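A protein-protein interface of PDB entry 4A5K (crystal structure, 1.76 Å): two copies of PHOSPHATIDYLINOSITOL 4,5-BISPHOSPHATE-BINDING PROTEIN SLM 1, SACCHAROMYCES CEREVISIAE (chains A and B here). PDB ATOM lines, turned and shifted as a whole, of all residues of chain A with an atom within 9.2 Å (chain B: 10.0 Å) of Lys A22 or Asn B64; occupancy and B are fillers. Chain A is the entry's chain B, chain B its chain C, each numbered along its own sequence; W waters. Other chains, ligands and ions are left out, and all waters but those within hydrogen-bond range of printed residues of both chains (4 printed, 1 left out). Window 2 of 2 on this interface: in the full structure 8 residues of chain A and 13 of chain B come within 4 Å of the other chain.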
ATOM      1  N   GLY A   8     -11.484 -35.599 -20.282  1.00  0.00           N
ATOM      2  CA  GLY A   8     -11.873 -35.059 -18.996  1.00  0.00           C
ATOM      3  C   GLY A   8     -13.101 -34.208 -19.141  1.00  0.00           C
ATOM      4  O   GLY A   8     -13.564 -33.961 -20.263  1.00  0.00           O
ATOM      5  N   PHE A   9     -13.649 -33.754 -18.019  1.00  0.00           N
ATOM      6  CA  PHE A   9     -14.805 -32.874 -18.073  1.00  0.00           C
ATOM      7  C   PHE A   9     -14.378 -31.449 -18.381  1.00  0.00           C
ATOM      8  O   PHE A   9     -13.355 -30.964 -17.873  1.00  0.00           O
ATOM      9  CB  PHE A   9     -15.565 -32.920 -16.748  1.00  0.00           C
ATOM     10  CG  PHE A   9     -16.171 -34.258 -16.468  1.00  0.00           C
ATOM     11  CD1 PHE A   9     -15.443 -35.235 -15.813  1.00  0.00           C
ATOM     12  CD2 PHE A   9     -17.441 -34.553 -16.921  1.00  0.00           C
ATOM     13  CE1 PHE A   9     -16.004 -36.472 -15.584  1.00  0.00           C
ATOM     14  CE2 PHE A   9     -18.009 -35.786 -16.687  1.00  0.00           C
ATOM     15  CZ  PHE A   9     -17.290 -36.738 -16.023  1.00  0.00           C
ATOM     16  N   LEU A  10     -15.162 -30.789 -19.228  1.00  0.00           N
ATOM     17  CA  LEU A  10     -15.010 -29.348 -19.464  1.00  0.00           C
ATOM     18  C   LEU A  10     -16.393 -28.728 -19.441  1.00  0.00           C
ATOM     19  O   LEU A  10     -17.387 -29.389 -19.750  1.00  0.00           O
ATOM     20  CB  LEU A  10     -14.410 -29.078 -20.848  1.00  0.00           C
ATOM     21  CG  LEU A  10     -12.978 -29.538 -21.119  1.00  0.00           C
ATOM     22  CD1 LEU A  10     -12.638 -29.357 -22.595  1.00  0.00           C
ATOM     23  CD2 LEU A  10     -12.064 -28.713 -20.239  1.00  0.00           C
ATOM     24  N   GLU A  11     -16.459 -27.447 -19.098  1.00  0.00           N
ATOM     25  CA  GLU A  11     -17.693 -26.701 -19.286  1.00  0.00           C
ATOM     26  C   GLU A  11     -17.557 -25.870 -20.544  1.00  0.00           C
ATOM     27  O   GLU A  11     -16.505 -25.290 -20.792  1.00  0.00           O
ATOM     28  CB  GLU A  11     -17.951 -25.789 -18.097  1.00  0.00           C
ATOM     29  CG  GLU A  11     -18.149 -26.545 -16.792  1.00  0.00           C
ATOM     30  CD  GLU A  11     -18.196 -25.600 -15.614  1.00  0.00           C
ATOM     31  OE1 GLU A  11     -19.207 -24.887 -15.476  1.00  0.00           O
ATOM     32  OE2 GLU A  11     -17.214 -25.548 -14.836  1.00  0.00           O
ATOM     33  N   ARG A  12     -18.611 -25.827 -21.342  1.00  0.00           N
ATOM     34  CA  ARG A  12     -18.580 -25.080 -22.603  1.00  0.00           C
ATOM     35  C   ARG A  12     -19.566 -23.930 -22.518  1.00  0.00           C
ATOM     36  O   ARG A  12     -20.716 -24.117 -22.125  1.00  0.00           O
ATOM     37  CB  ARG A  12     -18.883 -25.957 -23.813  1.00  0.00           C
ATOM     38  CG  ARG A  12     -18.787 -25.194 -25.125  1.00  0.00           C
ATOM     39  CD  ARG A  12     -18.789 -26.108 -26.338  1.00  0.00           C
ATOM     40  NE  ARG A  12     -19.726 -27.219 -26.205  1.00  0.00           N
ATOM     41  CZ  ARG A  12     -21.000 -27.179 -26.575  1.00  0.00           C
ATOM     42  NH1 ARG A  12     -21.504 -26.074 -27.098  1.00  0.00           N
ATOM     43  NH2 ARG A  12     -21.774 -28.244 -26.418  1.00  0.00           N
ATOM     44  N   ARG A  13     -19.110 -22.729 -22.848  1.00  0.00           N
ATOM     45  CA  ARG A  13     -19.979 -21.556 -22.711  1.00  0.00           C
ATOM     46  C   ARG A  13     -20.905 -21.399 -23.912  1.00  0.00           C
ATOM     47  O   ARG A  13     -20.521 -21.677 -25.057  1.00  0.00           O
ATOM     48  CB  ARG A  13     -19.128 -20.281 -22.566  1.00  0.00           C
ATOM     49  CG  ARG A  13     -19.919 -19.099 -21.990  1.00  0.00           C
ATOM     50  CD  ARG A  13     -19.024 -17.880 -21.788  1.00  0.00           C
ATOM     51  NE  ARG A  13     -19.782 -16.746 -21.259  1.00  0.00           N
ATOM     52  CZ  ARG A  13     -20.222 -15.733 -21.999  1.00  0.00           C
ATOM     53  NH1 ARG A  13     -19.972 -15.702 -23.302  1.00  0.00           N
ATOM     54  NH2 ARG A  13     -20.904 -14.745 -21.436  1.00  0.00           N
ATOM     55  N   SER A  14     -22.131 -20.936 -23.648  1.00  0.00           N
ATOM     56  CA  SER A  14     -23.038 -20.494 -24.696  1.00  0.00           C
ATOM     57  C   SER A  14     -22.995 -18.975 -24.737  1.00  0.00           C
ATOM     58  O   SER A  14     -23.281 -18.303 -23.744  1.00  0.00           O
ATOM     59  CB  SER A  14     -24.482 -20.935 -24.415  1.00  0.00           C
ATOM     60  OG  SER A  14     -25.378 -20.244 -25.284  1.00  0.00           O
ATOM     61  N   SER A  19     -24.416 -18.999 -20.237  1.00  0.00           N
ATOM     62  CA  SER A  19     -24.359 -20.045 -19.241  1.00  0.00           C
ATOM     63  C   SER A  19     -23.350 -21.074 -19.709  1.00  0.00           C
ATOM     64  O   SER A  19     -22.967 -21.088 -20.882  1.00  0.00           O
ATOM     65  CB  SER A  19     -25.713 -20.733 -19.118  1.00  0.00           C
ATOM     66  OG  SER A  19     -26.134 -21.166 -20.391  1.00  0.00           O
ATOM     67  N   TYR A  20     -22.954 -21.949 -18.792  1.00  0.00           N
ATOM     68  CA  TYR A  20     -22.054 -23.044 -19.124  1.00  0.00           C
ATOM     69  C   TYR A  20     -22.784 -24.346 -18.998  1.00  0.00           C
ATOM     70  O   TYR A  20     -23.677 -24.497 -18.168  1.00  0.00           O
ATOM     71  CB  TYR A  20     -20.856 -23.102 -18.179  1.00  0.00           C
ATOM     72  CG  TYR A  20     -19.829 -22.050 -18.465  1.00  0.00           C
ATOM     73  CD1 TYR A  20     -19.944 -20.788 -17.910  1.00  0.00           C
ATOM     74  CD2 TYR A  20     -18.753 -22.313 -19.319  1.00  0.00           C
ATOM     75  CE1 TYR A  20     -19.013 -19.808 -18.170  1.00  0.00           C
ATOM     76  CE2 TYR A  20     -17.811 -21.336 -19.576  1.00  0.00           C
ATOM     77  CZ  TYR A  20     -17.959 -20.083 -19.003  1.00  0.00           C
ATOM     78  OH  TYR A  20     -17.040 -19.091 -19.255  1.00  0.00           O
ATOM     79  N   SER A  21     -22.389 -25.291 -19.833  1.00  0.00           N
ATOM     80  CA  SER A  21     -22.870 -26.651 -19.694  1.00  0.00           C
ATOM     81  C   SER A  21     -21.704 -27.637 -19.671  1.00  0.00           C
ATOM     82  O   SER A  21     -20.840 -27.608 -20.539  1.00  0.00           O
ATOM     83  CB  SER A  21     -23.826 -27.000 -20.819  1.00  0.00           C
ATOM     84  OG  SER A  21     -24.296 -28.327 -20.632  1.00  0.00           O
ATOM     85  N   LYS A  22     -21.679 -28.504 -18.663  1.00  0.00           N
ATOM     86  CA  LYS A  22     -20.589 -29.471 -18.530  1.00  0.00           C
ATOM     87  C   LYS A  22     -20.780 -30.708 -19.417  1.00  0.00           C
ATOM     88  O   LYS A  22     -21.880 -31.249 -19.536  1.00  0.00           O
ATOM     89  CB  LYS A  22     -20.448 -29.886 -17.064  1.00  0.00           C
ATOM     90  CG  LYS A  22     -19.191 -30.653 -16.744  1.00  0.00           C
ATOM     91  CD  LYS A  22     -19.029 -30.769 -15.240  1.00  0.00           C
ATOM     92  CE  LYS A  22     -19.828 -31.945 -14.699  1.00  0.00           C
ATOM     93  NZ  LYS A  22     -19.940 -31.868 -13.220  1.00  0.00           N
ATOM     94  N   GLY A  23     -19.699 -31.151 -20.047  1.00  0.00           N
ATOM     95  CA  GLY A  23     -19.712 -32.382 -20.801  1.00  0.00           C
ATOM     96  C   GLY A  23     -18.421 -33.150 -20.610  1.00  0.00           C
ATOM     97  O   GLY A  23     -17.469 -32.645 -20.019  1.00  0.00           O
ATOM     98  N   TYR A  24     -18.384 -34.376 -21.109  1.00  0.00           N
ATOM     99  CA  TYR A  24     -17.172 -35.160 -21.056  1.00  0.00           C
ATOM    100  C   TYR A  24     -16.469 -35.158 -22.408  1.00  0.00           C
ATOM    101  O   TYR A  24     -17.036 -35.603 -23.393  1.00  0.00           O
ATOM    102  CB  TYR A  24     -17.462 -36.593 -20.642  1.00  0.00           C
ATOM    103  CG  TYR A  24     -16.191 -37.287 -20.276  1.00  0.00           C
ATOM    104  CD1 TYR A  24     -15.627 -37.104 -19.017  1.00  0.00           C
ATOM    105  CD2 TYR A  24     -15.519 -38.077 -21.194  1.00  0.00           C
ATOM    106  CE1 TYR A  24     -14.449 -37.711 -18.673  1.00  0.00           C
ATOM    107  CE2 TYR A  24     -14.328 -38.699 -20.853  1.00  0.00           C
ATOM    108  CZ  TYR A  24     -13.807 -38.508 -19.583  1.00  0.00           C
ATOM    109  OH  TYR A  24     -12.631 -39.114 -19.228  1.00  0.00           O
ATOM    110  N   TYR A  25     -15.247 -34.637 -22.457  1.00  0.00           N
ATOM    111  CA  TYR A  25     -14.568 -34.432 -23.740  1.00  0.00           C
ATOM    112  C   TYR A  25     -13.419 -35.392 -23.953  1.00  0.00           C
ATOM    113  O   TYR A  25     -12.691 -35.743 -23.013  1.00  0.00           O
ATOM    114  CB  TYR A  25     -14.088 -32.964 -23.869  1.00  0.00           C
ATOM    115  CG  TYR A  25     -15.236 -32.011 -24.061  1.00  0.00           C
ATOM    116  CD1 TYR A  25     -16.015 -31.614 -22.994  1.00  0.00           C
ATOM    117  CD2 TYR A  25     -15.561 -31.531 -25.328  1.00  0.00           C
ATOM    118  CE1 TYR A  25     -17.097 -30.767 -23.170  1.00  0.00           C
ATOM    119  CE2 TYR A  25     -16.623 -30.673 -25.511  1.00  0.00           C
ATOM    120  CZ  TYR A  25     -17.385 -30.294 -24.437  1.00  0.00           C
ATOM    121  OH  TYR A  25     -18.445 -29.445 -24.612  1.00  0.00           O
ATOM    122  N   GLU A  34     -17.315 -34.558 -27.879  1.00  0.00           N
ATOM    123  CA  GLU A  34     -18.089 -34.349 -26.663  1.00  0.00           C
ATOM    124  C   GLU A  34     -18.962 -35.584 -26.431  1.00  0.00           C
ATOM    125  O   GLU A  34     -19.632 -36.048 -27.348  1.00  0.00           O
ATOM    126  CB  GLU A  34     -19.010 -33.130 -26.786  1.00  0.00           C
ATOM    127  CG  GLU A  34     -19.792 -32.909 -25.507  1.00  0.00           C
ATOM    128  CD  GLU A  34     -20.911 -31.893 -25.647  1.00  0.00           C
ATOM    129  OE1 GLU A  34     -21.057 -31.287 -26.729  1.00  0.00           O
ATOM    130  OE2 GLU A  34     -21.646 -31.703 -24.659  1.00  0.00           O
ATOM    131  N   PHE A  35     -18.943 -36.116 -25.212  1.00  0.00           N
ATOM    132  CA  PHE A  35     -19.833 -37.223 -24.835  1.00  0.00           C
ATOM    133  C   PHE A  35     -20.607 -36.802 -23.587  1.00  0.00           C
ATOM    134  O   PHE A  35     -20.215 -35.868 -22.911  1.00  0.00           O
ATOM    135  CB  PHE A  35     -19.023 -38.462 -24.475  1.00  0.00           C
ATOM    136  CG  PHE A  35     -18.318 -39.091 -25.623  1.00  0.00           C
ATOM    137  CD1 PHE A  35     -18.967 -40.029 -26.408  1.00  0.00           C
ATOM    138  CD2 PHE A  35     -16.994 -38.787 -25.896  1.00  0.00           C
ATOM    139  CE1 PHE A  35     -18.309 -40.653 -27.454  1.00  0.00           C
ATOM    140  CE2 PHE A  35     -16.329 -39.409 -26.942  1.00  0.00           C
ATOM    141  CZ  PHE A  35     -16.996 -40.334 -27.732  1.00  0.00           C
ATOM    142  N   LYS A  36     -21.691 -37.497 -23.262  1.00  0.00           N
ATOM    143  CA  LYS A  36     -22.466 -37.125 -22.075  1.00  0.00           C
ATOM    144  C   LYS A  36     -21.811 -37.615 -20.784  1.00  0.00           C
ATOM    145  O   LYS A  36     -21.956 -36.989 -19.728  1.00  0.00           O
ATOM    146  CB  LYS A  36     -23.906 -37.634 -22.167  1.00  0.00           C
ATOM    147  CG  LYS A  36     -24.709 -36.956 -23.270  1.00  0.00           C
ATOM    148  CD  LYS A  36     -26.207 -37.120 -23.072  1.00  0.00           C
ATOM    149  CE  LYS A  36     -26.972 -36.651 -24.303  1.00  0.00           C
ATOM    150  NZ  LYS A  36     -26.652 -35.238 -24.651  1.00  0.00           N
ATOM    151  N   THR A  37     -21.073 -38.716 -20.878  1.00  0.00           N
ATOM    152  CA  THR A  37     -20.458 -39.325 -19.694  1.00  0.00           C
ATOM    153  C   THR A  37     -19.071 -39.853 -19.986  1.00  0.00           C
ATOM    154  O   THR A  37     -18.650 -39.931 -21.143  1.00  0.00           O
ATOM    155  CB  THR A  37     -21.280 -40.526 -19.168  1.00  0.00           C
ATOM    156  OG1 THR A  37     -21.065 -41.657 -20.021  1.00  0.00           O
ATOM    157  CG2 THR A  37     -22.765 -40.183 -19.078  1.00  0.00           C
ATOM    158  N   VAL A  47     -21.848 -36.582 -28.786  1.00  0.00           N
ATOM    159  CA  VAL A  47     -22.838 -35.526 -28.919  1.00  0.00           C
ATOM    160  C   VAL A  47     -22.436 -34.633 -30.082  1.00  0.00           C
ATOM    161  O   VAL A  47     -23.286 -34.100 -30.811  1.00  0.00           O
ATOM    162  CB  VAL A  47     -22.913 -34.684 -27.632  1.00  0.00           C
ATOM    163  CG1 VAL A  47     -23.748 -33.426 -27.853  1.00  0.00           C
ATOM    164  CG2 VAL A  47     -23.449 -35.529 -26.480  1.00  0.00           C
ATOM    165  N   PHE A  96     -14.144 -22.607 -23.471  1.00  0.00           N
ATOM    166  CA  PHE A  96     -14.200 -23.745 -22.560  1.00  0.00           C
ATOM    167  C   PHE A  96     -13.576 -23.406 -21.229  1.00  0.00           C
ATOM    168  O   PHE A  96     -12.626 -22.628 -21.157  1.00  0.00           O
ATOM    169  CB  PHE A  96     -13.448 -24.930 -23.151  1.00  0.00           C
ATOM    170  CG  PHE A  96     -14.097 -25.502 -24.367  1.00  0.00           C
ATOM    171  CD1 PHE A  96     -13.804 -25.005 -25.627  1.00  0.00           C
ATOM    172  CD2 PHE A  96     -15.004 -26.546 -24.253  1.00  0.00           C
ATOM    173  CE1 PHE A  96     -14.410 -25.531 -26.759  1.00  0.00           C
ATOM    174  CE2 PHE A  96     -15.604 -27.081 -25.391  1.00  0.00           C
ATOM    175  CZ  PHE A  96     -15.310 -26.573 -26.638  1.00  0.00           C
ATOM    176  N   LYS A  97     -14.107 -24.014 -20.176  1.00  0.00           N
ATOM    177  CA  LYS A  97     -13.594 -23.825 -18.825  1.00  0.00           C
ATOM    178  C   LYS A  97     -13.216 -25.185 -18.235  1.00  0.00           C
ATOM    179  O   LYS A  97     -14.055 -26.083 -18.131  1.00  0.00           O
ATOM    180  CB  LYS A  97     -14.657 -23.135 -17.958  1.00  0.00           C
ATOM    181  CG  LYS A  97     -14.208 -22.893 -16.521  1.00  0.00           C
ATOM    182  CD  LYS A  97     -15.330 -22.343 -15.653  1.00  0.00           C
ATOM    183  CE  LYS A  97     -15.731 -20.925 -16.061  1.00  0.00           C
ATOM    184  NZ  LYS A  97     -16.794 -20.389 -15.149  1.00  0.00           N
ATOM    185  N   ALA A  98     -11.945 -25.337 -17.885  1.00  0.00           N
ATOM    186  CA  ALA A  98     -11.427 -26.562 -17.258  1.00  0.00           C
ATOM    187  C   ALA A  98     -11.500 -26.454 -15.732  1.00  0.00           C
ATOM    188  O   ALA A  98     -11.931 -25.437 -15.192  1.00  0.00           O
ATOM    189  CB  ALA A  98      -9.992 -26.805 -17.697  1.00  0.00           C
ATOM    190  N   ASP A  99     -11.041 -27.488 -15.027  1.00  0.00           N
ATOM    191  CA  ASP A  99     -11.222 -27.524 -13.574  1.00  0.00           C
ATOM    192  C   ASP A  99     -10.088 -26.845 -12.793  1.00  0.00           C
ATOM    193  O   ASP A  99     -10.154 -26.719 -11.574  1.00  0.00           O
ATOM    194  CB  ASP A  99     -11.477 -28.961 -13.082  1.00  0.00           C
ATOM    195  CG  ASP A  99     -10.343 -29.912 -13.408  1.00  0.00           C
ATOM    196  OD1 ASP A  99      -9.200 -29.449 -13.585  1.00  0.00           O
ATOM    197  OD2 ASP A  99     -10.594 -31.134 -13.487  1.00  0.00           O
ATOM    198  N   HIS B  60     -31.150 -23.868 -26.605  1.00  0.00           N
ATOM    199  CA  HIS B  60     -31.821 -23.746 -25.326  1.00  0.00           C
ATOM    200  C   HIS B  60     -30.917 -24.279 -24.224  1.00  0.00           C
ATOM    201  O   HIS B  60     -29.947 -25.006 -24.483  1.00  0.00           O
ATOM    202  CB  HIS B  60     -33.197 -24.437 -25.369  1.00  0.00           C
ATOM    203  CG  HIS B  60     -33.130 -25.928 -25.519  1.00  0.00           C
ATOM    204  ND1 HIS B  60     -32.711 -26.756 -24.501  1.00  0.00           N
ATOM    205  CD2 HIS B  60     -33.460 -26.740 -26.552  1.00  0.00           C
ATOM    206  CE1 HIS B  60     -32.772 -28.014 -24.903  1.00  0.00           C
ATOM    207  NE2 HIS B  60     -33.231 -28.035 -26.142  1.00  0.00           N
ATOM    208  N   SER B  61     -31.214 -23.880 -23.000  1.00  0.00           N
ATOM    209  CA  SER B  61     -30.452 -24.289 -21.842  1.00  0.00           C
ATOM    210  C   SER B  61     -30.502 -25.801 -21.705  1.00  0.00           C
ATOM    211  O   SER B  61     -31.494 -26.421 -22.065  1.00  0.00           O
ATOM    212  CB  SER B  61     -31.070 -23.666 -20.590  1.00  0.00           C
ATOM    213  OG  SER B  61     -31.118 -22.244 -20.669  1.00  0.00           O
ATOM    214  N   ARG B  62     -29.437 -26.393 -21.179  1.00  0.00           N
ATOM    215  CA  ARG B  62     -29.497 -27.801 -20.799  1.00  0.00           C
ATOM    216  C   ARG B  62     -29.875 -27.868 -19.327  1.00  0.00           C
ATOM    217  O   ARG B  62     -29.740 -26.886 -18.595  1.00  0.00           O
ATOM    218  CB  ARG B  62     -28.165 -28.500 -21.088  1.00  0.00           C
ATOM    219  CG  ARG B  62     -27.848 -28.603 -22.579  1.00  0.00           C
ATOM    220  CD  ARG B  62     -26.662 -29.523 -22.843  1.00  0.00           C
ATOM    221  NE  ARG B  62     -26.787 -30.775 -22.102  1.00  0.00           N
ATOM    222  CZ  ARG B  62     -25.833 -31.290 -21.332  1.00  0.00           C
ATOM    223  NH1 ARG B  62     -24.668 -30.671 -21.210  1.00  0.00           N
ATOM    224  NH2 ARG B  62     -26.041 -32.429 -20.693  1.00  0.00           N
ATOM    225  N   LYS B  63     -30.371 -29.013 -18.877  1.00  0.00           N
ATOM    226  CA  LYS B  63     -30.829 -29.084 -17.500  1.00  0.00           C
ATOM    227  C   LYS B  63     -29.685 -28.771 -16.541  1.00  0.00           C
ATOM    228  O   LYS B  63     -29.914 -28.272 -15.441  1.00  0.00           O
ATOM    229  CB  LYS B  63     -31.433 -30.459 -17.194  1.00  0.00           C
ATOM    230  CG  LYS B  63     -32.524 -30.409 -16.131  1.00  0.00           C
ATOM    231  CD  LYS B  63     -33.138 -31.778 -15.851  1.00  0.00           C
ATOM    232  CE  LYS B  63     -33.861 -32.347 -17.063  1.00  0.00           C
ATOM    233  NZ  LYS B  63     -32.923 -32.848 -18.108  1.00  0.00           N
ATOM    234  N   ASN B  64     -28.450 -29.026 -16.980  1.00  0.00           N
ATOM    235  CA  ASN B  64     -27.272 -28.737 -16.152  1.00  0.00           C
ATOM    236  C   ASN B  64     -26.635 -27.356 -16.377  1.00  0.00           C
ATOM    237  O   ASN B  64     -25.569 -27.059 -15.835  1.00  0.00           O
ATOM    238  CB  ASN B  64     -26.209 -29.845 -16.304  1.00  0.00           C
ATOM    239  CG  ASN B  64     -25.377 -29.706 -17.570  1.00  0.00           C
ATOM    240  OD1 ASN B  64     -25.691 -28.909 -18.465  1.00  0.00           O
ATOM    241  ND2 ASN B  64     -24.302 -30.490 -17.651  1.00  0.00           N
ATOM    242  N   SER B  65     -27.285 -26.508 -17.166  1.00  0.00           N
ATOM    243  CA  SER B  65     -26.719 -25.188 -17.466  1.00  0.00           C
ATOM    244  C   SER B  65     -26.633 -24.297 -16.235  1.00  0.00           C
ATOM    245  O   SER B  65     -27.569 -24.235 -15.442  1.00  0.00           O
ATOM    246  CB  SER B  65     -27.538 -24.497 -18.558  1.00  0.00           C
ATOM    247  OG  SER B  65     -27.197 -25.032 -19.836  1.00  0.00           O
ATOM    248  N   THR B  66     -25.516 -23.589 -16.089  1.00  0.00           N
ATOM    249  CA  THR B  66     -25.283 -22.768 -14.902  1.00  0.00           C
ATOM    250  C   THR B  66     -24.815 -21.376 -15.286  1.00  0.00           C
ATOM    251  O   THR B  66     -24.241 -21.184 -16.355  1.00  0.00           O
ATOM    252  CB  THR B  66     -24.194 -23.373 -14.016  1.00  0.00           C
ATOM    253  OG1 THR B  66     -22.981 -23.462 -14.773  1.00  0.00           O
ATOM    254  CG2 THR B  66     -24.603 -24.760 -13.537  1.00  0.00           C
ATOM    255  N   SER B  67     -25.039 -20.417 -14.394  1.00  0.00           N
ATOM    256  CA  SER B  67     -24.720 -19.020 -14.676  1.00  0.00           C
ATOM    257  C   SER B  67     -24.032 -18.346 -13.495  1.00  0.00           C
ATOM    258  O   SER B  67     -23.014 -18.835 -12.996  1.00  0.00           O
ATOM    259  CB  SER B  67     -25.984 -18.247 -15.074  1.00  0.00           C
ATOM    260  OG  SER B  67     -27.038 -18.465 -14.142  1.00  0.00           O
ATOM    261  N   GLY B  73     -32.900 -18.864 -13.610  1.00  0.00           N
ATOM    262  CA  GLY B  73     -33.317 -19.416 -14.885  1.00  0.00           C
ATOM    263  C   GLY B  73     -32.191 -19.859 -15.795  1.00  0.00           C
ATOM    264  O   GLY B  73     -32.364 -19.892 -17.012  1.00  0.00           O
ATOM    265  N   SER B  74     -31.045 -20.221 -15.221  1.00  0.00           N
ATOM    266  CA  SER B  74     -29.910 -20.623 -16.045  1.00  0.00           C
ATOM    267  C   SER B  74     -30.242 -21.875 -16.841  1.00  0.00           C
ATOM    268  O   SER B  74     -29.607 -22.162 -17.858  1.00  0.00           O
ATOM    269  CB  SER B  74     -28.644 -20.837 -15.200  1.00  0.00           C
ATOM    270  OG  SER B  74     -28.742 -22.001 -14.399  1.00  0.00           O
ATOM    271  N   ASP B  75     -31.250 -22.609 -16.379  1.00  0.00           N
ATOM    272  CA  ASP B  75     -31.692 -23.817 -17.050  1.00  0.00           C
ATOM    273  C   ASP B  75     -33.010 -23.608 -17.783  1.00  0.00           C
ATOM    274  O   ASP B  75     -33.672 -24.583 -18.141  1.00  0.00           O
ATOM    275  CB  ASP B  75     -31.861 -24.964 -16.042  1.00  0.00           C
ATOM    276  CG  ASP B  75     -32.894 -24.659 -14.958  1.00  0.00           C
ATOM    277  OD1 ASP B  75     -33.350 -23.500 -14.857  1.00  0.00           O
ATOM    278  OD2 ASP B  75     -33.254 -25.592 -14.202  1.00  0.00           O
ATOM    279  N   ALA B  76     -33.385 -22.353 -18.024  1.00  0.00           N
ATOM    280  CA  ALA B  76     -34.726 -22.076 -18.542  1.00  0.00           C
ATOM    281  C   ALA B  76     -34.772 -21.070 -19.706  1.00  0.00           C
ATOM    282  O   ALA B  76     -35.793 -20.398 -19.915  1.00  0.00           O
ATOM    283  CB  ALA B  76     -35.608 -21.599 -17.395  1.00  0.00           C
ATOM    284  N   TYR B 101     -36.992 -25.212 -16.360  1.00  0.00           N
ATOM    285  CA  TYR B 101     -36.574 -26.016 -17.490  1.00  0.00           C
ATOM    286  C   TYR B 101     -37.750 -26.626 -18.242  1.00  0.00           C
ATOM    287  O   TYR B 101     -37.808 -26.585 -19.464  1.00  0.00           O
ATOM    288  CB  TYR B 101     -35.623 -27.128 -17.027  1.00  0.00           C
ATOM    289  CG  TYR B 101     -35.199 -28.050 -18.148  1.00  0.00           C
ATOM    290  CD1 TYR B 101     -34.200 -27.675 -19.044  1.00  0.00           C
ATOM    291  CD2 TYR B 101     -35.798 -29.297 -18.316  1.00  0.00           C
ATOM    292  CE1 TYR B 101     -33.804 -28.516 -20.061  1.00  0.00           C
ATOM    293  CE2 TYR B 101     -35.409 -30.142 -19.332  1.00  0.00           C
ATOM    294  CZ  TYR B 101     -34.414 -29.747 -20.201  1.00  0.00           C
ATOM    295  OH  TYR B 101     -34.028 -30.580 -21.217  1.00  0.00           O
ATOM    296  N   MET B 104     -39.663 -23.991 -20.127  1.00  0.00           N
ATOM    297  CA  MET B 104     -38.874 -23.602 -21.285  1.00  0.00           C
ATOM    298  C   MET B 104     -38.988 -24.631 -22.400  1.00  0.00           C
ATOM    299  O   MET B 104     -39.164 -24.279 -23.561  1.00  0.00           O
ATOM    300  CB  MET B 104     -37.395 -23.395 -20.898  1.00  0.00           C
ATOM    301  CG  MET B 104     -36.487 -23.078 -22.104  1.00  0.00           C
ATOM    302  SD  MET B 104     -35.925 -24.590 -22.943  1.00  0.00           S
ATOM    303  CE  MET B 104     -34.822 -25.175 -21.661  1.00  0.00           C
HETATM  304  O   HOH W   1     -21.655 -25.656 -15.495  1.00  0.00           O
HETATM  305  O   HOH W   2     -25.458 -23.651 -21.447  1.00  0.00           O
HETATM  306  O   HOH W   3     -22.967 -27.703 -16.016  1.00  0.00           O
HETATM  307  O   HOH W   4     -28.831 -20.767 -19.850  1.00  0.00           O
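The side-chain amide oxygen of Asn B64 sits at hydrogen-bond distance from the side-chain hydroxyl of Ser A21.
O of Lys A22 is in hydrogen-bond range of ND2 of Asn B64, 3.2 Å away.
The guanidinium group (NH1) of Arg B62 is in hydrogen-bond range of the backbone carbonyl oxygen (O) of Lys A22 (3.3 Å).
The backbone NH (N) of Tyr A20 lies within hydrogen-bond range of the backbone carbonyl oxygen (O) of Thr B66 (2.9 Å).
NH1 of Arg B62 lies within hydrogen-bond range of OG of Ser A21 (2.4 Å).
NH1 of Arg B62 lies within hydrogen-bond range of OD1 of Asn B64, 3.4 Å away.
The backbone NH (N) of Ser A14 lies within hydrogen-bond range of the backbone carbonyl oxygen (O) of Ser A19 (2.9 Å).
O of Ser B65 sits at hydrogen-bond distance from OG of Ser B74.
The backbone carbonyl oxygen (O) of Ser A21 lies within hydrogen-bond range of the backbone NH (N) of Arg A12 (3.0 Å).
The backbone NH of Arg B62 sits at hydrogen-bond distance from the side-chain hydroxyl of Ser B65 (2.9 Å).
Among the printed residues, merely in contact across the chains: Ser A19 with Thr B66 (3.1 Å), Tyr A20 with Asn B64 (3.9 Å) and Tyr A20 with Ser B65 (3.2 Å).
Of the printed residues of chain B, Ser A19 touches Thr B66.
Of the printed residues of chain B, Tyr A20 touches Asn B64, Ser B65 and Thr B66.
Of the printed residues of chain B, Ser A21 touches Arg B62 and Asn B64.
No residue of chain B comes within 4 Å of Gly A23.
Tyr A25 touches none of the printed residues of chain B.
Lys B63 touches none of the printed residues of chain A.
Asn B64 touches just these residues of chain A: Tyr A20 (3.9 Å), Ser A21 (2.6 Å) and Lys A22 (3.2 Å).
Of chain A, only Tyr A20 comes within 4 Å of Ser B65.
Of the printed residues of chain A, Thr B66 touches Ser A19 (3.1 Å) and Tyr A20 (2.9 Å).
The nearest printed residue of chain A that does not touch Thr B66 is Glu A11 (4.1 Å).
Among the printed residues, no Asp or Glu carboxylate lies within 4 Å of a Lys or Arg side-chain nitrogen of the other chain.
No position is printed for both chains.
Water W4 lies within hydrogen-bond range of O of Ser B74 (2.6 Å), OG of Ser A19 (2.8 Å) and OG of Ser B61 (2.8 Å).
Water W1 bridges OE1 of Glu A11 (2.6 Å) and OG1 of Thr B66 (2.7 Å).
Water W3 bridges the backbone carbonyl oxygen of Asn B64 (2.7 Å) and the backbone NH of Lys A22 (3.1 Å).
Water W2 bridges the side-chain hydroxyl of Ser B65 (2.7 Å) and the side-chain hydroxyl of Ser A19 (2.8 Å).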
